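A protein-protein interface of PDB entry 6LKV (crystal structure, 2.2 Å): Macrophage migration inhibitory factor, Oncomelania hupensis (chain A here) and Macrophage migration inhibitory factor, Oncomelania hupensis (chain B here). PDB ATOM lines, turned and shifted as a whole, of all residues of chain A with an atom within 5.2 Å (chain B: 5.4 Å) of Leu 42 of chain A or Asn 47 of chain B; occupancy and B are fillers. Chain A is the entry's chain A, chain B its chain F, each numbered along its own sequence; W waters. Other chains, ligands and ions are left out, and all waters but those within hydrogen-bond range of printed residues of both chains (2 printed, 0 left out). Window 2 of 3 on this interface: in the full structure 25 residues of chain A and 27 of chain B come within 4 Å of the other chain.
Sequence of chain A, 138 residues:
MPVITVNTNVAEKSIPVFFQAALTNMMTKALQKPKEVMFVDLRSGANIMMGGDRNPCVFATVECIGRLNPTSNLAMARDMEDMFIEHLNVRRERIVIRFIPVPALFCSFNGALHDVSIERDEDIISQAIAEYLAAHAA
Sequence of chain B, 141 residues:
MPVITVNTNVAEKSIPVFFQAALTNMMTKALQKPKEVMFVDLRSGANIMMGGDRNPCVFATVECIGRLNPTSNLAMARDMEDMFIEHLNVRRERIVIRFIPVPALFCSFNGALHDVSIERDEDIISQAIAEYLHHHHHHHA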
ATOM      1  N   VAL A   6       4.342 -14.372 -34.555  1.00  0.00           N
ATOM      2  CA  VAL A   6       3.765 -15.747 -34.597  1.00  0.00           C
ATOM      3  C   VAL A   6       2.334 -15.628 -35.112  1.00  0.00           C
ATOM      4  O   VAL A   6       1.539 -14.974 -34.451  1.00  0.00           O
ATOM      5  CB  VAL A   6       3.841 -16.400 -33.220  1.00  0.00           C
ATOM      6  CG1 VAL A   6       3.261 -17.796 -33.249  1.00  0.00           C
ATOM      7  CG2 VAL A   6       5.263 -16.414 -32.676  1.00  0.00           C
ATOM      8  N   THR A   8      -0.816 -17.820 -35.982  1.00  0.00           N
ATOM      9  CA  THR A   8      -1.345 -19.170 -35.684  1.00  0.00           C
ATOM     10  C   THR A   8      -2.869 -19.107 -35.558  1.00  0.00           C
ATOM     11  O   THR A   8      -3.391 -18.118 -35.015  1.00  0.00           O
ATOM     12  CB  THR A   8      -0.718 -19.765 -34.423  1.00  0.00           C
ATOM     13  OG1 THR A   8      -1.180 -21.110 -34.333  1.00  0.00           O
ATOM     14  CG2 THR A   8      -1.034 -19.015 -33.149  1.00  0.00           C
ATOM     15  N   GLU A  12      -6.199 -17.805 -28.759  1.00  0.00           N
ATOM     16  CA  GLU A  12      -5.457 -17.025 -27.732  1.00  0.00           C
ATOM     17  C   GLU A  12      -5.663 -17.630 -26.351  1.00  0.00           C
ATOM     18  O   GLU A  12      -4.675 -17.795 -25.615  1.00  0.00           O
ATOM     19  CB  GLU A  12      -5.963 -15.586 -27.737  1.00  0.00           C
ATOM     20  CG  GLU A  12      -5.173 -14.636 -26.862  1.00  0.00           C
ATOM     21  CD  GLU A  12      -5.685 -13.216 -27.060  1.00  0.00           C
ATOM     22  OE1 GLU A  12      -5.335 -12.567 -28.113  1.00  0.00           O
ATOM     23  OE2 GLU A  12      -6.505 -12.783 -26.215  1.00  0.00           O
ATOM     24  N   ILE A  15      -3.508 -20.587 -25.123  1.00  0.00           N
ATOM     25  CA  ILE A  15      -2.022 -20.461 -25.164  1.00  0.00           C
ATOM     26  C   ILE A  15      -1.552 -20.107 -23.759  1.00  0.00           C
ATOM     27  O   ILE A  15      -2.104 -19.206 -23.138  1.00  0.00           O
ATOM     28  CB  ILE A  15      -1.606 -19.421 -26.225  1.00  0.00           C
ATOM     29  CG1 ILE A  15      -1.918 -19.968 -27.620  1.00  0.00           C
ATOM     30  CG2 ILE A  15      -0.135 -19.024 -26.060  1.00  0.00           C
ATOM     31  CD1 ILE A  15      -1.776 -18.957 -28.745  1.00  0.00           C
ATOM     32  N   PHE A  19       3.826 -17.592 -22.613  1.00  0.00           N
ATOM     33  CA  PHE A  19       4.393 -18.076 -23.891  1.00  0.00           C
ATOM     34  C   PHE A  19       5.261 -16.963 -24.501  1.00  0.00           C
ATOM     35  O   PHE A  19       6.400 -17.223 -24.849  1.00  0.00           O
ATOM     36  CB  PHE A  19       3.290 -18.509 -24.848  1.00  0.00           C
ATOM     37  CG  PHE A  19       3.814 -18.890 -26.197  1.00  0.00           C
ATOM     38  CD1 PHE A  19       4.509 -20.075 -26.356  1.00  0.00           C
ATOM     39  CD2 PHE A  19       3.576 -18.091 -27.304  1.00  0.00           C
ATOM     40  CE1 PHE A  19       5.006 -20.427 -27.605  1.00  0.00           C
ATOM     41  CE2 PHE A  19       4.072 -18.449 -28.542  1.00  0.00           C
ATOM     42  CZ  PHE A  19       4.791 -19.602 -28.688  1.00  0.00           C
ATOM     43  N   GLN A  20       4.733 -15.753 -24.605  1.00  0.00           N
ATOM     44  CA  GLN A  20       5.451 -14.610 -25.232  1.00  0.00           C
ATOM     45  C   GLN A  20       6.688 -14.249 -24.397  1.00  0.00           C
ATOM     46  O   GLN A  20       7.759 -14.022 -25.003  1.00  0.00           O
ATOM     47  CB  GLN A  20       4.492 -13.434 -25.388  1.00  0.00           C
ATOM     48  CG  GLN A  20       3.535 -13.608 -26.545  1.00  0.00           C
ATOM     49  CD  GLN A  20       2.436 -12.587 -26.434  1.00  0.00           C
ATOM     50  OE1 GLN A  20       1.482 -12.814 -25.693  1.00  0.00           O
ATOM     51  NE2 GLN A  20       2.557 -11.475 -27.166  1.00  0.00           N
ATOM     52  N   VAL A  40       7.741  -9.528 -29.317  1.00  0.00           N
ATOM     53  CA  VAL A  40       6.984 -10.736 -29.727  1.00  0.00           C
ATOM     54  C   VAL A  40       5.538 -10.324 -29.992  1.00  0.00           C
ATOM     55  O   VAL A  40       4.830  -9.842 -29.044  1.00  0.00           O
ATOM     56  CB  VAL A  40       7.093 -11.870 -28.703  1.00  0.00           C
ATOM     57  CG1 VAL A  40       6.355 -13.094 -29.192  1.00  0.00           C
ATOM     58  CG2 VAL A  40       8.545 -12.190 -28.371  1.00  0.00           C
ATOM     59  N   ASP A  41       5.128 -10.485 -31.245  1.00  0.00           N
ATOM     60  CA  ASP A  41       3.766 -10.163 -31.729  1.00  0.00           C
ATOM     61  C   ASP A  41       3.066 -11.493 -31.955  1.00  0.00           C
ATOM     62  O   ASP A  41       3.393 -12.163 -32.950  1.00  0.00           O
ATOM     63  CB  ASP A  41       3.807  -9.304 -32.992  1.00  0.00           C
ATOM     64  CG  ASP A  41       2.452  -8.773 -33.430  1.00  0.00           C
ATOM     65  OD1 ASP A  41       1.440  -9.097 -32.778  1.00  0.00           O
ATOM     66  OD2 ASP A  41       2.422  -8.014 -34.408  1.00  0.00           O
ATOM     67  N   LEU A  42       2.152 -11.869 -31.054  1.00  0.00           N
ATOM     68  CA  LEU A  42       1.397 -13.142 -31.179  1.00  0.00           C
ATOM     69  C   LEU A  42       0.046 -12.829 -31.830  1.00  0.00           C
ATOM     70  O   LEU A  42      -0.790 -12.162 -31.221  1.00  0.00           O
ATOM     71  CB  LEU A  42       1.258 -13.797 -29.809  1.00  0.00           C
ATOM     72  CG  LEU A  42       0.383 -15.039 -29.759  1.00  0.00           C
ATOM     73  CD1 LEU A  42       0.903 -16.129 -30.678  1.00  0.00           C
ATOM     74  CD2 LEU A  42       0.285 -15.540 -28.325  1.00  0.00           C
ATOM     75  N   ARG A  43      -0.112 -13.249 -33.073  1.00  0.00           N
ATOM     76  CA  ARG A  43      -1.389 -13.192 -33.803  1.00  0.00           C
ATOM     77  C   ARG A  43      -2.032 -14.577 -33.701  1.00  0.00           C
ATOM     78  O   ARG A  43      -1.886 -15.384 -34.611  1.00  0.00           O
ATOM     79  CB  ARG A  43      -1.132 -12.733 -35.227  1.00  0.00           C
ATOM     80  CG  ARG A  43      -0.299 -11.474 -35.260  1.00  0.00           C
ATOM     81  CD  ARG A  43      -0.398 -10.871 -36.620  1.00  0.00           C
ATOM     82  NE  ARG A  43       0.483  -9.712 -36.655  1.00  0.00           N
ATOM     83  CZ  ARG A  43       1.396  -9.495 -37.578  1.00  0.00           C
ATOM     84  NH1 ARG A  43       1.546 -10.364 -38.573  1.00  0.00           N
ATOM     85  NH2 ARG A  43       2.102  -8.382 -37.523  1.00  0.00           N
ATOM     86  N   SER A  44      -2.683 -14.818 -32.578  1.00  0.00           N
ATOM     87  CA  SER A  44      -3.369 -16.093 -32.282  1.00  0.00           C
ATOM     88  C   SER A  44      -4.812 -15.922 -32.735  1.00  0.00           C
ATOM     89  O   SER A  44      -5.243 -14.751 -32.984  1.00  0.00           O
ATOM     90  CB  SER A  44      -3.208 -16.478 -30.831  1.00  0.00           C
ATOM     91  OG  SER A  44      -3.786 -15.508 -30.005  1.00  0.00           O
ATOM     92  N   GLY B  45      -4.630  -2.736 -30.502  1.00  0.00           N
ATOM     93  CA  GLY B  45      -5.005  -3.819 -29.574  1.00  0.00           C
ATOM     94  C   GLY B  45      -4.261  -5.095 -29.911  1.00  0.00           C
ATOM     95  O   GLY B  45      -4.731  -6.166 -29.525  1.00  0.00           O
ATOM     96  N   ALA B  46      -3.116  -4.995 -30.604  1.00  0.00           N
ATOM     97  CA  ALA B  46      -2.286  -6.165 -30.945  1.00  0.00           C
ATOM     98  C   ALA B  46      -1.742  -6.788 -29.657  1.00  0.00           C
ATOM     99  O   ALA B  46      -1.404  -6.078 -28.740  1.00  0.00           O
ATOM    100  CB  ALA B  46      -1.161  -5.813 -31.896  1.00  0.00           C
ATOM    101  N   ASN B  47      -1.604  -8.091 -29.663  1.00  0.00           N
ATOM    102  CA  ASN B  47      -0.918  -8.858 -28.610  1.00  0.00           C
ATOM    103  C   ASN B  47       0.581  -8.793 -28.891  1.00  0.00           C
ATOM    104  O   ASN B  47       1.200  -9.821 -29.228  1.00  0.00           O
ATOM    105  CB  ASN B  47      -1.458 -10.272 -28.542  1.00  0.00           C
ATOM    106  CG  ASN B  47      -0.966 -10.986 -27.307  1.00  0.00           C
ATOM    107  OD1 ASN B  47      -0.232 -10.411 -26.499  1.00  0.00           O
ATOM    108  ND2 ASN B  47      -1.322 -12.253 -27.215  1.00  0.00           N
ATOM    109  N   ILE B  48       1.138  -7.592 -28.762  1.00  0.00           N
ATOM    110  CA  ILE B  48       2.572  -7.332 -29.019  1.00  0.00           C
ATOM    111  C   ILE B  48       3.177  -6.821 -27.716  1.00  0.00           C
ATOM    112  O   ILE B  48       2.612  -5.904 -27.121  1.00  0.00           O
ATOM    113  CB  ILE B  48       2.775  -6.377 -30.215  1.00  0.00           C
ATOM    114  CG1 ILE B  48       4.265  -6.239 -30.552  1.00  0.00           C
ATOM    115  CG2 ILE B  48       2.124  -5.025 -29.991  1.00  0.00           C
ATOM    116  CD1 ILE B  48       4.522  -5.563 -31.883  1.00  0.00           C
ATOM    117  N   MET B  49       4.223  -7.470 -27.254  1.00  0.00           N
ATOM    118  CA  MET B  49       5.015  -7.014 -26.092  1.00  0.00           C
ATOM    119  C   MET B  49       6.436  -6.691 -26.578  1.00  0.00           C
ATOM    120  O   MET B  49       6.869  -7.166 -27.678  1.00  0.00           O
ATOM    121  CB  MET B  49       5.061  -8.066 -24.983  1.00  0.00           C
ATOM    122  CG  MET B  49       5.641  -9.392 -25.396  1.00  0.00           C
ATOM    123  SD  MET B  49       6.114 -10.416 -23.952  1.00  0.00           S
ATOM    124  CE  MET B  49       4.548 -10.541 -23.107  1.00  0.00           C
ATOM    125  N   ARG B  54       4.456  -5.131 -21.272  1.00  0.00           N
ATOM    126  CA  ARG B  54       3.217  -4.758 -21.998  1.00  0.00           C
ATOM    127  C   ARG B  54       2.945  -3.265 -21.875  1.00  0.00           C
ATOM    128  O   ARG B  54       1.824  -2.858 -22.217  1.00  0.00           O
ATOM    129  CB  ARG B  54       2.023  -5.611 -21.561  1.00  0.00           C
ATOM    130  CG  ARG B  54       2.205  -7.097 -21.850  1.00  0.00           C
ATOM    131  CD  ARG B  54       0.902  -7.857 -21.755  1.00  0.00           C
ATOM    132  NE  ARG B  54       1.038  -9.260 -22.108  1.00  0.00           N
ATOM    133  CZ  ARG B  54       0.925  -9.772 -23.328  1.00  0.00           C
ATOM    134  NH1 ARG B  54       0.697  -9.000 -24.377  1.00  0.00           N
ATOM    135  NH2 ARG B  54       1.033 -11.074 -23.516  1.00  0.00           N
HETATM  136  O   HOH W   1      -3.229 -13.153 -29.419  1.00  0.00           O
HETATM  137  O   HOH W   2      -1.216  -9.479 -32.209  1.00  0.00           O
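The side-chain amide nitrogen of Gln 20 of chain A is in hydrogen-bond range of the backbone carbonyl oxygen of Asn 47 of chain B (3.0 Å).
The backbone carbonyl oxygen of Asn 47 of chain B sits at hydrogen-bond distance from the backbone NH of Leu 42 of chain A (2.9 Å).
The side-chain amide oxygen of Gln 20 of chain A lies within hydrogen-bond range of the guanidinium group of Arg 54 of chain B.
The backbone NH (N) of Val 40 of chain A sits at hydrogen-bond distance from the backbone carbonyl oxygen (O) of Met 49 of chain B (3.0 Å).
N of Val 6 of chain A is in hydrogen-bond range of O of Asp 41 of chain A.
The side-chain amide oxygen of Asn 47 of chain B is in hydrogen-bond range of the guanidinium group of Arg 54 of chain B, 2.7 Å away.
The backbone carbonyl oxygen (O) of Val 40 of chain A is in hydrogen-bond range of the side-chain amide nitrogen (NE2) of Gln 20 of chain A (3.4 Å).
The guanidinium group (NH2) of Arg 43 of chain A is in salt-bridge range of the side-chain carboxylate (OD2) of Asp 41 of chain A.
Gln 20 of chain A touches Met 49 of chain B.
Val 40 of chain A touches Asn 47 of chain B (O to O, 3.6 Å).
Val 40 of chain A touches Ile 48 of chain B.
Asp 41 of chain A touches Asn 47 of chain B (CA to O, 3.6 Å).
Ile 48 of chain B touches Asp 41 of chain A (CG1 to CB, 3.9 Å).
Of the printed residues of chain B, Gln 20 of chain A touches Asn 47, Met 49 and Arg 54.
Of the printed residues of chain B, Val 40 of chain A touches Asn 47 (3.6 Å), Ile 48 (3.4 Å) and Met 49 (3.0 Å).
Of the printed residues of chain B, Asp 41 of chain A touches Asn 47 and Ile 48.
Asn 47 of chain B touches just these residues of chain A: Gln 20 (3.0 Å), Val 40 (3.6 Å), Asp 41 (3.6 Å) and Leu 42 (2.9 Å).
Printed residues of chain A within 4 Å of Ile 48 of chain B: Val 40 and Asp 41.
Printed residues of chain A within 4 Å of Arg 54 of chain B: Gln 20.
The nearest residue of chain B that does not touch Leu 42 of chain A is Ile 48 of chain B (5.0 Å).
The nearest printed residue of chain A that does not touch Met 49 of chain B is Asp 41 of chain A (5.1 Å).
Hydrophobic or aromatic side chains of chain B that line the printed part of chain A: Ile 48 and Met 49.
Of the 11 printed residues of chain A, 4 touch a printed residue of chain B.
Printed residues of chain A that touch a printed residue of chain B: Gln 20, Val 40, Asp 41 and Leu 42.
Among the printed residues, no Asp or Glu carboxylate lies within 4 Å of a Lys or Arg side-chain nitrogen of the other chain.
Water W1 lies within hydrogen-bond range of the side-chain hydroxyl (OG) of Ser 44 of chain A (2.5 Å), the side-chain carboxylate (OE1) of Glu 12 of chain A (2.5 Å), the side-chain amide nitrogen (ND2) of Asn 47 of chain B (3.1 Å) and the backbone carbonyl oxygen (O) of Leu 42 of chain A (3.2 Å).
Water W2 lies within hydrogen-bond range of the side-chain carboxylate (OD1) of Asp 41 of chain A (2.7 Å), the backbone carbonyl oxygen (O) of Leu 42 of chain A (2.9 Å) and the backbone NH (N) of Asn 47 of chain B (2.9 Å).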
